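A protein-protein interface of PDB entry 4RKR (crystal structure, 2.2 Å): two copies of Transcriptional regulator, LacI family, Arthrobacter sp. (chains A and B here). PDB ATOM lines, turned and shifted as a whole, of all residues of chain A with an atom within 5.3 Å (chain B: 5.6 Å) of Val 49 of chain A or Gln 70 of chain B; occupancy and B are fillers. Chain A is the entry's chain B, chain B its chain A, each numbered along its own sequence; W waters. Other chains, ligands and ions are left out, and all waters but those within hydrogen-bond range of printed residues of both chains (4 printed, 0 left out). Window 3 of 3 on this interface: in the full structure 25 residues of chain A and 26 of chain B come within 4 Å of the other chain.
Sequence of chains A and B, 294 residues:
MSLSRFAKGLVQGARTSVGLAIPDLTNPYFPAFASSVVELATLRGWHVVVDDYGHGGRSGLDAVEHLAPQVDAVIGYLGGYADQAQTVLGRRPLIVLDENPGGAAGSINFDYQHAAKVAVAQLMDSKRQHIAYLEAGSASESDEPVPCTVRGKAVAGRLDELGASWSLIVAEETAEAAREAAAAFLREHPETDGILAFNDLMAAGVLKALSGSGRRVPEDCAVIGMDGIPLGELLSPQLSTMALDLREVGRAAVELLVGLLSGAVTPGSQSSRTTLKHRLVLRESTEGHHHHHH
O of Val 50 of chain A lies within hydrogen-bond range of N of Val 50 of chain B, at 2.9 Å.
The side-chain amide oxygen (OE1) of Gln 70 of chain B lies close to the side-chain amide oxygen (OE1) of Gln 70 of chain A, at 3.4 Å.
The side-chain hydroxyl (OG) of Ser 17 of chain A lies within hydrogen-bond range of the backbone carbonyl oxygen (O) of Gln 70 of chain A (2.9 Å).
The side-chain amide nitrogen (NE2) of Gln 70 of chain B lies within hydrogen-bond range of the backbone carbonyl oxygen (O) of His 66 of chain B (3.3 Å).
The backbone carbonyl oxygen (O) of Gln 70 of chain B is in hydrogen-bond range of the side-chain hydroxyl (OG) of Ser 17 of chain B, at 2.9 Å.
A ring nitrogen (ND1) of His 66 of chain B sits at hydrogen-bond distance from the side-chain carboxylate (OD2) of Asp 51 of chain B.
The backbone carbonyl oxygen (O) of His 47 of chain A is in hydrogen-bond range of the backbone NH (N) of Val 18 of chain A (2.8 Å).
The backbone NH of Leu 20 of chain A sits at hydrogen-bond distance from the backbone carbonyl oxygen of Val 49 of chain A (2.8 Å).
Among the printed residues, merely in contact across the chains: Val 49 of chain A with His 66 of chain B, His 47 of chain A with His 66 of chain B, Val 48 of chain A with His 66 of chain B, Val 50 of chain A with Val 49 of chain B, Val 49 of chain A with Val 50 of chain B and Val 49 of chain A with Gln 70 of chain B.
Printed residues of chain B within 4 Å of Val 49 of chain A: Val 50, His 66 and Gln 70.
Printed residues of chain A within 4 Å of Gln 70 of chain B: Val 49 (3.998 Å) and Gln 70 (3.1 Å).
Printed residues of chain A within 4 Å of His 66 of chain B: His 47, Val 48 and Val 49.
Of the printed residues of chain B, Gln 70 of chain A touches Gln 70 (3.1 Å).
Printed residues of chain A within 4 Å of Val 50 of chain B: Val 49 and Val 50.
Of the printed residues of chain B, Val 50 of chain A touches Val 49 and Val 50.
Pro 69 of chain B touches none of the printed residues of chain A.
The nearest printed residue of chain A that does not touch His 66 of chain B is Ser 17 of chain A (4.8 Å).
Hydrophobic or aromatic side chains of chain A that line the printed part of chain B: His 47, Val 49 and Val 50.
Hydrophobic or aromatic side chains of chain B that line the printed part of chain A: Val 50 and His 66.
Among the printed residues, 8 pairs touch across the chains.
Val 49 of chain A touches Val 50 of chain B, and with the chains exchanged Val 50 of chain A touches Val 49 of chain B.
Val 49 of chain A touches Gln 70 of chain B, but with the chains exchanged Gln 70 of chain A does not touch Val 49 of chain B (6.3 Å).
Val 50 of chain B touches its own counterpart, Val 50 of chain A.
Gln 70 of chain A touches its own counterpart, Gln 70 of chain B.
Of the 8 pairs that touch across the chains among the printed residues, 4 have their exchanged pair printed and touching as well.
Water W3 lies within hydrogen-bond range of the side-chain carboxylate (OD1) of Asp 51 of chain B (2.4 Å) and the backbone carbonyl oxygen (O) of Val 48 of chain A (2.9 Å).
Water W1 lies within hydrogen-bond range of OG of Ser 17 of chain A (2.7 Å), NE2 of Gln 70 of chain B (3.0 Å) and NE2 of His 66 of chain B (3.1 Å).
Water W4 lies within hydrogen-bond range of the backbone NH of Val 48 of chain A (3.0 Å) and the side-chain carboxylate of Asp 51 of chain B (3.4 Å).
Water W2 bridges O of Val 50 of chain B (3.1 Å) and O of Val 48 of chain A (3.4 Å).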
ATOM      1  N   SER A  17      -3.475   1.293 -25.602  1.00  0.00           N
ATOM      2  CA  SER A  17      -2.984   0.233 -24.757  1.00  0.00           C
ATOM      3  C   SER A  17      -1.779  -0.399 -25.461  1.00  0.00           C
ATOM      4  O   SER A  17      -1.811  -0.658 -26.655  1.00  0.00           O
ATOM      5  CB  SER A  17      -4.097  -0.797 -24.528  1.00  0.00           C
ATOM      6  OG  SER A  17      -3.674  -1.844 -23.674  1.00  0.00           O
ATOM      7  N   VAL A  18      -0.711  -0.636 -24.716  1.00  0.00           N
ATOM      8  CA  VAL A  18       0.493  -1.190 -25.293  1.00  0.00           C
ATOM      9  C   VAL A  18       0.935  -2.398 -24.500  1.00  0.00           C
ATOM     10  O   VAL A  18       1.010  -2.345 -23.272  1.00  0.00           O
ATOM     11  CB  VAL A  18       1.612  -0.151 -25.316  1.00  0.00           C
ATOM     12  CG1 VAL A  18       2.881  -0.751 -25.889  1.00  0.00           C
ATOM     13  CG2 VAL A  18       1.162   1.056 -26.126  1.00  0.00           C
ATOM     14  N   GLY A  19       1.200  -3.488 -25.214  1.00  0.00           N
ATOM     15  CA  GLY A  19       1.675  -4.726 -24.614  1.00  0.00           C
ATOM     16  C   GLY A  19       3.194  -4.705 -24.494  1.00  0.00           C
ATOM     17  O   GLY A  19       3.874  -4.274 -25.402  1.00  0.00           O
ATOM     18  N   LEU A  20       3.722  -5.162 -23.362  1.00  0.00           N
ATOM     19  CA  LEU A  20       5.159  -5.192 -23.139  1.00  0.00           C
ATOM     20  C   LEU A  20       5.540  -6.621 -22.796  1.00  0.00           C
ATOM     21  O   LEU A  20       5.099  -7.165 -21.780  1.00  0.00           O
ATOM     22  CB  LEU A  20       5.522  -4.230 -22.009  1.00  0.00           C
ATOM     23  CG  LEU A  20       7.002  -3.968 -21.759  1.00  0.00           C
ATOM     24  CD1 LEU A  20       7.742  -3.616 -23.039  1.00  0.00           C
ATOM     25  CD2 LEU A  20       7.133  -2.848 -20.741  1.00  0.00           C
ATOM     26  N   HIS A  47      -1.915   3.111 -21.600  1.00  0.00           N
ATOM     27  CA  HIS A  47      -1.899   1.994 -20.674  1.00  0.00           C
ATOM     28  C   HIS A  47      -0.880   1.009 -21.177  1.00  0.00           C
ATOM     29  O   HIS A  47      -0.666   0.901 -22.387  1.00  0.00           O
ATOM     30  CB  HIS A  47      -3.277   1.331 -20.567  1.00  0.00           C
ATOM     31  CG  HIS A  47      -4.161   1.935 -19.517  1.00  0.00           C
ATOM     32  ND1 HIS A  47      -5.511   2.142 -19.707  1.00  0.00           N
ATOM     33  CD2 HIS A  47      -3.887   2.375 -18.263  1.00  0.00           C
ATOM     34  CE1 HIS A  47      -6.032   2.673 -18.616  1.00  0.00           C
ATOM     35  NE2 HIS A  47      -5.068   2.826 -17.723  1.00  0.00           N
ATOM     36  N   VAL A  48      -0.224   0.337 -20.239  1.00  0.00           N
ATOM     37  CA  VAL A  48       0.728  -0.711 -20.553  1.00  0.00           C
ATOM     38  C   VAL A  48       0.423  -1.942 -19.731  1.00  0.00           C
ATOM     39  O   VAL A  48       0.202  -1.838 -18.522  1.00  0.00           O
ATOM     40  CB  VAL A  48       2.169  -0.282 -20.250  1.00  0.00           C
ATOM     41  CG1 VAL A  48       3.140  -1.389 -20.625  1.00  0.00           C
ATOM     42  CG2 VAL A  48       2.504   0.981 -21.016  1.00  0.00           C
ATOM     43  N   VAL A  49       0.398  -3.098 -20.394  1.00  0.00           N
ATOM     44  CA  VAL A  49       0.317  -4.392 -19.700  1.00  0.00           C
ATOM     45  C   VAL A  49       1.563  -5.174 -20.019  1.00  0.00           C
ATOM     46  O   VAL A  49       2.010  -5.216 -21.169  1.00  0.00           O
ATOM     47  CB  VAL A  49      -0.926  -5.218 -20.066  1.00  0.00           C
ATOM     48  CG1 VAL A  49      -2.151  -4.629 -19.390  1.00  0.00           C
ATOM     49  CG2 VAL A  49      -1.123  -5.293 -21.573  1.00  0.00           C
ATOM     50  N   VAL A  50       2.141  -5.768 -18.990  1.00  0.00           N
ATOM     51  CA  VAL A  50       3.396  -6.460 -19.136  1.00  0.00           C
ATOM     52  C   VAL A  50       3.111  -7.937 -19.089  1.00  0.00           C
ATOM     53  O   VAL A  50       2.372  -8.420 -18.225  1.00  0.00           O
ATOM     54  CB  VAL A  50       4.377  -6.087 -18.012  1.00  0.00           C
ATOM     55  CG1 VAL A  50       5.649  -6.918 -18.109  1.00  0.00           C
ATOM     56  CG2 VAL A  50       4.724  -4.610 -18.072  1.00  0.00           C
ATOM     57  N   ASP A  51       3.705  -8.662 -20.016  1.00  0.00           N
ATOM     58  CA  ASP A  51       3.647 -10.112 -19.957  1.00  0.00           C
ATOM     59  C   ASP A  51       5.078 -10.637 -19.816  1.00  0.00           C
ATOM     60  O   ASP A  51       5.881 -10.567 -20.755  1.00  0.00           O
ATOM     61  CB  ASP A  51       2.947 -10.680 -21.196  1.00  0.00           C
ATOM     62  CG  ASP A  51       2.742 -12.187 -21.117  1.00  0.00           C
ATOM     63  OD1 ASP A  51       3.293 -12.808 -20.198  1.00  0.00           O
ATOM     64  OD2 ASP A  51       2.034 -12.764 -21.971  1.00  0.00           O
ATOM     65  N   LEU A  67      -1.494 -10.987 -25.648  1.00  0.00           N
ATOM     66  CA  LEU A  67      -1.667  -9.537 -25.534  1.00  0.00           C
ATOM     67  C   LEU A  67      -2.474  -8.887 -26.648  1.00  0.00           C
ATOM     68  O   LEU A  67      -3.086  -7.842 -26.437  1.00  0.00           O
ATOM     69  CB  LEU A  67      -0.288  -8.860 -25.501  1.00  0.00           C
ATOM     70  CG  LEU A  67       0.613  -9.200 -24.306  1.00  0.00           C
ATOM     71  CD1 LEU A  67       2.007  -8.633 -24.524  1.00  0.00           C
ATOM     72  CD2 LEU A  67       0.017  -8.696 -22.998  1.00  0.00           C
ATOM     73  N   GLN A  70      -5.885  -7.192 -26.401  1.00  0.00           N
ATOM     74  CA  GLN A  70      -5.984  -6.120 -25.389  1.00  0.00           C
ATOM     75  C   GLN A  70      -5.153  -4.880 -25.725  1.00  0.00           C
ATOM     76  O   GLN A  70      -5.160  -3.899 -24.975  1.00  0.00           O
ATOM     77  CB  GLN A  70      -5.495  -6.635 -24.032  1.00  0.00           C
ATOM     78  CG  GLN A  70      -6.292  -7.789 -23.477  1.00  0.00           C
ATOM     79  CD  GLN A  70      -7.675  -7.376 -23.014  1.00  0.00           C
ATOM     80  OE1 GLN A  70      -8.040  -6.198 -23.038  1.00  0.00           O
ATOM     81  NE2 GLN A  70      -8.454  -8.353 -22.582  1.00  0.00           N
ATOM     82  N   VAL A  71      -4.407  -4.933 -26.820  1.00  0.00           N
ATOM     83  CA  VAL A  71      -3.430  -3.892 -27.121  1.00  0.00           C
ATOM     84  C   VAL A  71      -3.542  -3.405 -28.554  1.00  0.00           C
ATOM     85  O   VAL A  71      -4.037  -4.113 -29.434  1.00  0.00           O
ATOM     86  CB  VAL A  71      -1.990  -4.381 -26.885  1.00  0.00           C
ATOM     87  CG1 VAL A  71      -1.814  -4.848 -25.446  1.00  0.00           C
ATOM     88  CG2 VAL A  71      -1.624  -5.482 -27.861  1.00  0.00           C
ATOM     89  N   SER B  17      -7.910 -15.395 -16.112  1.00  0.00           N
ATOM     90  CA  SER B  17      -7.015 -14.267 -16.316  1.00  0.00           C
ATOM     91  C   SER B  17      -6.838 -13.506 -15.016  1.00  0.00           C
ATOM     92  O   SER B  17      -7.809 -13.013 -14.458  1.00  0.00           O
ATOM     93  CB  SER B  17      -7.601 -13.332 -17.371  1.00  0.00           C
ATOM     94  OG  SER B  17      -6.786 -12.194 -17.557  1.00  0.00           O
ATOM     95  N   VAL B  49      -1.350 -10.653 -16.461  1.00  0.00           N
ATOM     96  CA  VAL B  49      -0.827  -9.361 -16.909  1.00  0.00           C
ATOM     97  C   VAL B  49      -0.347  -8.569 -15.691  1.00  0.00           C
ATOM     98  O   VAL B  49      -1.003  -8.564 -14.640  1.00  0.00           O
ATOM     99  CB  VAL B  49      -1.860  -8.546 -17.725  1.00  0.00           C
ATOM    100  CG1 VAL B  49      -1.953  -9.079 -19.150  1.00  0.00           C
ATOM    101  CG2 VAL B  49      -3.237  -8.551 -17.068  1.00  0.00           C
ATOM    102  N   VAL B  50       0.815  -7.933 -15.823  1.00  0.00           N
ATOM    103  CA  VAL B  50       1.355  -7.083 -14.756  1.00  0.00           C
ATOM    104  C   VAL B  50       1.170  -5.610 -15.098  1.00  0.00           C
ATOM    105  O   VAL B  50       1.482  -5.174 -16.214  1.00  0.00           O
ATOM    106  CB  VAL B  50       2.845  -7.356 -14.506  1.00  0.00           C
ATOM    107  CG1 VAL B  50       3.393  -6.405 -13.442  1.00  0.00           C
ATOM    108  CG2 VAL B  50       3.039  -8.814 -14.111  1.00  0.00           C
ATOM    109  N   ASP B  51       0.615  -4.869 -14.141  1.00  0.00           N
ATOM    110  CA  ASP B  51       0.515  -3.415 -14.223  1.00  0.00           C
ATOM    111  C   ASP B  51       1.394  -2.803 -13.134  1.00  0.00           C
ATOM    112  O   ASP B  51       1.063  -2.856 -11.932  1.00  0.00           O
ATOM    113  CB  ASP B  51      -0.926  -2.954 -14.049  1.00  0.00           C
ATOM    114  CG  ASP B  51      -1.089  -1.450 -14.230  1.00  0.00           C
ATOM    115  OD1 ASP B  51      -0.090  -0.736 -14.453  1.00  0.00           O
ATOM    116  OD2 ASP B  51      -2.233  -0.971 -14.155  1.00  0.00           O
ATOM    117  N   HIS B  66      -7.758  -0.326 -14.449  1.00  0.00           N
ATOM    118  CA  HIS B  66      -7.196  -0.685 -15.761  1.00  0.00           C
ATOM    119  C   HIS B  66      -7.351  -2.193 -15.993  1.00  0.00           C
ATOM    120  O   HIS B  66      -7.748  -2.645 -17.060  1.00  0.00           O
ATOM    121  CB  HIS B  66      -5.725  -0.238 -15.820  1.00  0.00           C
ATOM    122  CG  HIS B  66      -4.954  -0.806 -16.960  1.00  0.00           C
ATOM    123  ND1 HIS B  66      -3.643  -1.213 -16.832  1.00  0.00           N
ATOM    124  CD2 HIS B  66      -5.304  -1.056 -18.243  1.00  0.00           C
ATOM    125  CE1 HIS B  66      -3.215  -1.681 -17.990  1.00  0.00           C
ATOM    126  NE2 HIS B  66      -4.206  -1.602 -18.862  1.00  0.00           N
ATOM    127  N   LEU B  67      -7.079  -2.964 -14.956  1.00  0.00           N
ATOM    128  CA  LEU B  67      -6.989  -4.415 -15.092  1.00  0.00           C
ATOM    129  C   LEU B  67      -8.331  -5.124 -15.132  1.00  0.00           C
ATOM    130  O   LEU B  67      -8.475  -6.139 -15.810  1.00  0.00           O
ATOM    131  CB  LEU B  67      -6.176  -4.976 -13.930  1.00  0.00           C
ATOM    132  CG  LEU B  67      -4.709  -4.592 -13.973  1.00  0.00           C
ATOM    133  CD1 LEU B  67      -4.013  -5.018 -12.693  1.00  0.00           C
ATOM    134  CD2 LEU B  67      -4.040  -5.196 -15.204  1.00  0.00           C
ATOM    135  N   ALA B  68      -9.297  -4.575 -14.401  1.00  0.00           N
ATOM    136  CA  ALA B  68     -10.570  -5.234 -14.133  1.00  0.00           C
ATOM    137  C   ALA B  68     -11.279  -5.829 -15.352  1.00  0.00           C
ATOM    138  O   ALA B  68     -11.636  -7.013 -15.342  1.00  0.00           O
ATOM    139  CB  ALA B  68     -11.504  -4.281 -13.396  1.00  0.00           C
ATOM    140  N   PRO B  69     -11.497  -5.019 -16.403  1.00  0.00           N
ATOM    141  CA  PRO B  69     -12.262  -5.552 -17.541  1.00  0.00           C
ATOM    142  C   PRO B  69     -11.572  -6.720 -18.262  1.00  0.00           C
ATOM    143  O   PRO B  69     -12.239  -7.491 -18.948  1.00  0.00           O
ATOM    144  CB  PRO B  69     -12.390  -4.364 -18.500  1.00  0.00           C
ATOM    145  CG  PRO B  69     -11.735  -3.193 -17.852  1.00  0.00           C
ATOM    146  CD  PRO B  69     -11.076  -3.619 -16.583  1.00  0.00           C
ATOM    147  N   GLN B  70     -10.251  -6.834 -18.130  1.00  0.00           N
ATOM    148  CA  GLN B  70      -9.508  -7.895 -18.827  1.00  0.00           C
ATOM    149  C   GLN B  70      -9.003  -8.976 -17.886  1.00  0.00           C
ATOM    150  O   GLN B  70      -8.200  -9.785 -18.301  1.00  0.00           O
ATOM    151  CB  GLN B  70      -8.352  -7.320 -19.663  1.00  0.00           C
ATOM    152  CG  GLN B  70      -7.278  -6.591 -18.866  1.00  0.00           C
ATOM    153  CD  GLN B  70      -6.338  -5.728 -19.713  1.00  0.00           C
ATOM    154  OE1 GLN B  70      -5.615  -6.223 -20.590  1.00  0.00           O
ATOM    155  NE2 GLN B  70      -6.318  -4.428 -19.420  1.00  0.00           N
ATOM    156  N   VAL B  71      -9.482  -9.011 -16.632  1.00  0.00           N
ATOM    157  CA  VAL B  71      -9.123 -10.079 -15.692  1.00  0.00           C
ATOM    158  C   VAL B  71     -10.314 -10.569 -14.884  1.00  0.00           C
ATOM    159  O   VAL B  71     -11.352  -9.921 -14.860  1.00  0.00           O
ATOM    160  CB  VAL B  71      -8.011  -9.651 -14.708  1.00  0.00           C
ATOM    161  CG1 VAL B  71      -6.778  -9.213 -15.472  1.00  0.00           C
ATOM    162  CG2 VAL B  71      -8.481  -8.554 -13.745  1.00  0.00           C
ATOM    163  N   ASP B  72     -10.138 -11.720 -14.225  1.00  0.00           N
ATOM    164  CA  ASP B  72     -11.165 -12.330 -13.387  1.00  0.00           C
ATOM    165  C   ASP B  72     -10.847 -12.119 -11.923  1.00  0.00           C
ATOM    166  O   ASP B  72     -11.673 -12.411 -11.061  1.00  0.00           O
ATOM    167  CB  ASP B  72     -11.260 -13.835 -13.663  1.00  0.00           C
ATOM    168  CG  ASP B  72     -11.561 -14.138 -15.101  1.00  0.00           C
ATOM    169  OD1 ASP B  72     -12.458 -13.478 -15.673  1.00  0.00           O
ATOM    170  OD2 ASP B  72     -10.892 -15.025 -15.666  1.00  0.00           O
HETATM  171  O   HOH W   1      -4.780  -2.975 -21.542  1.00  0.00           O
HETATM  172  O   HOH W   2       2.842  -2.431 -16.480  1.00  0.00           O
HETATM  173  O   HOH W   3       1.357  -0.366 -16.348  1.00  0.00           O
HETATM  174  O   HOH W   4      -0.859   0.944 -17.363  1.00  0.00           O
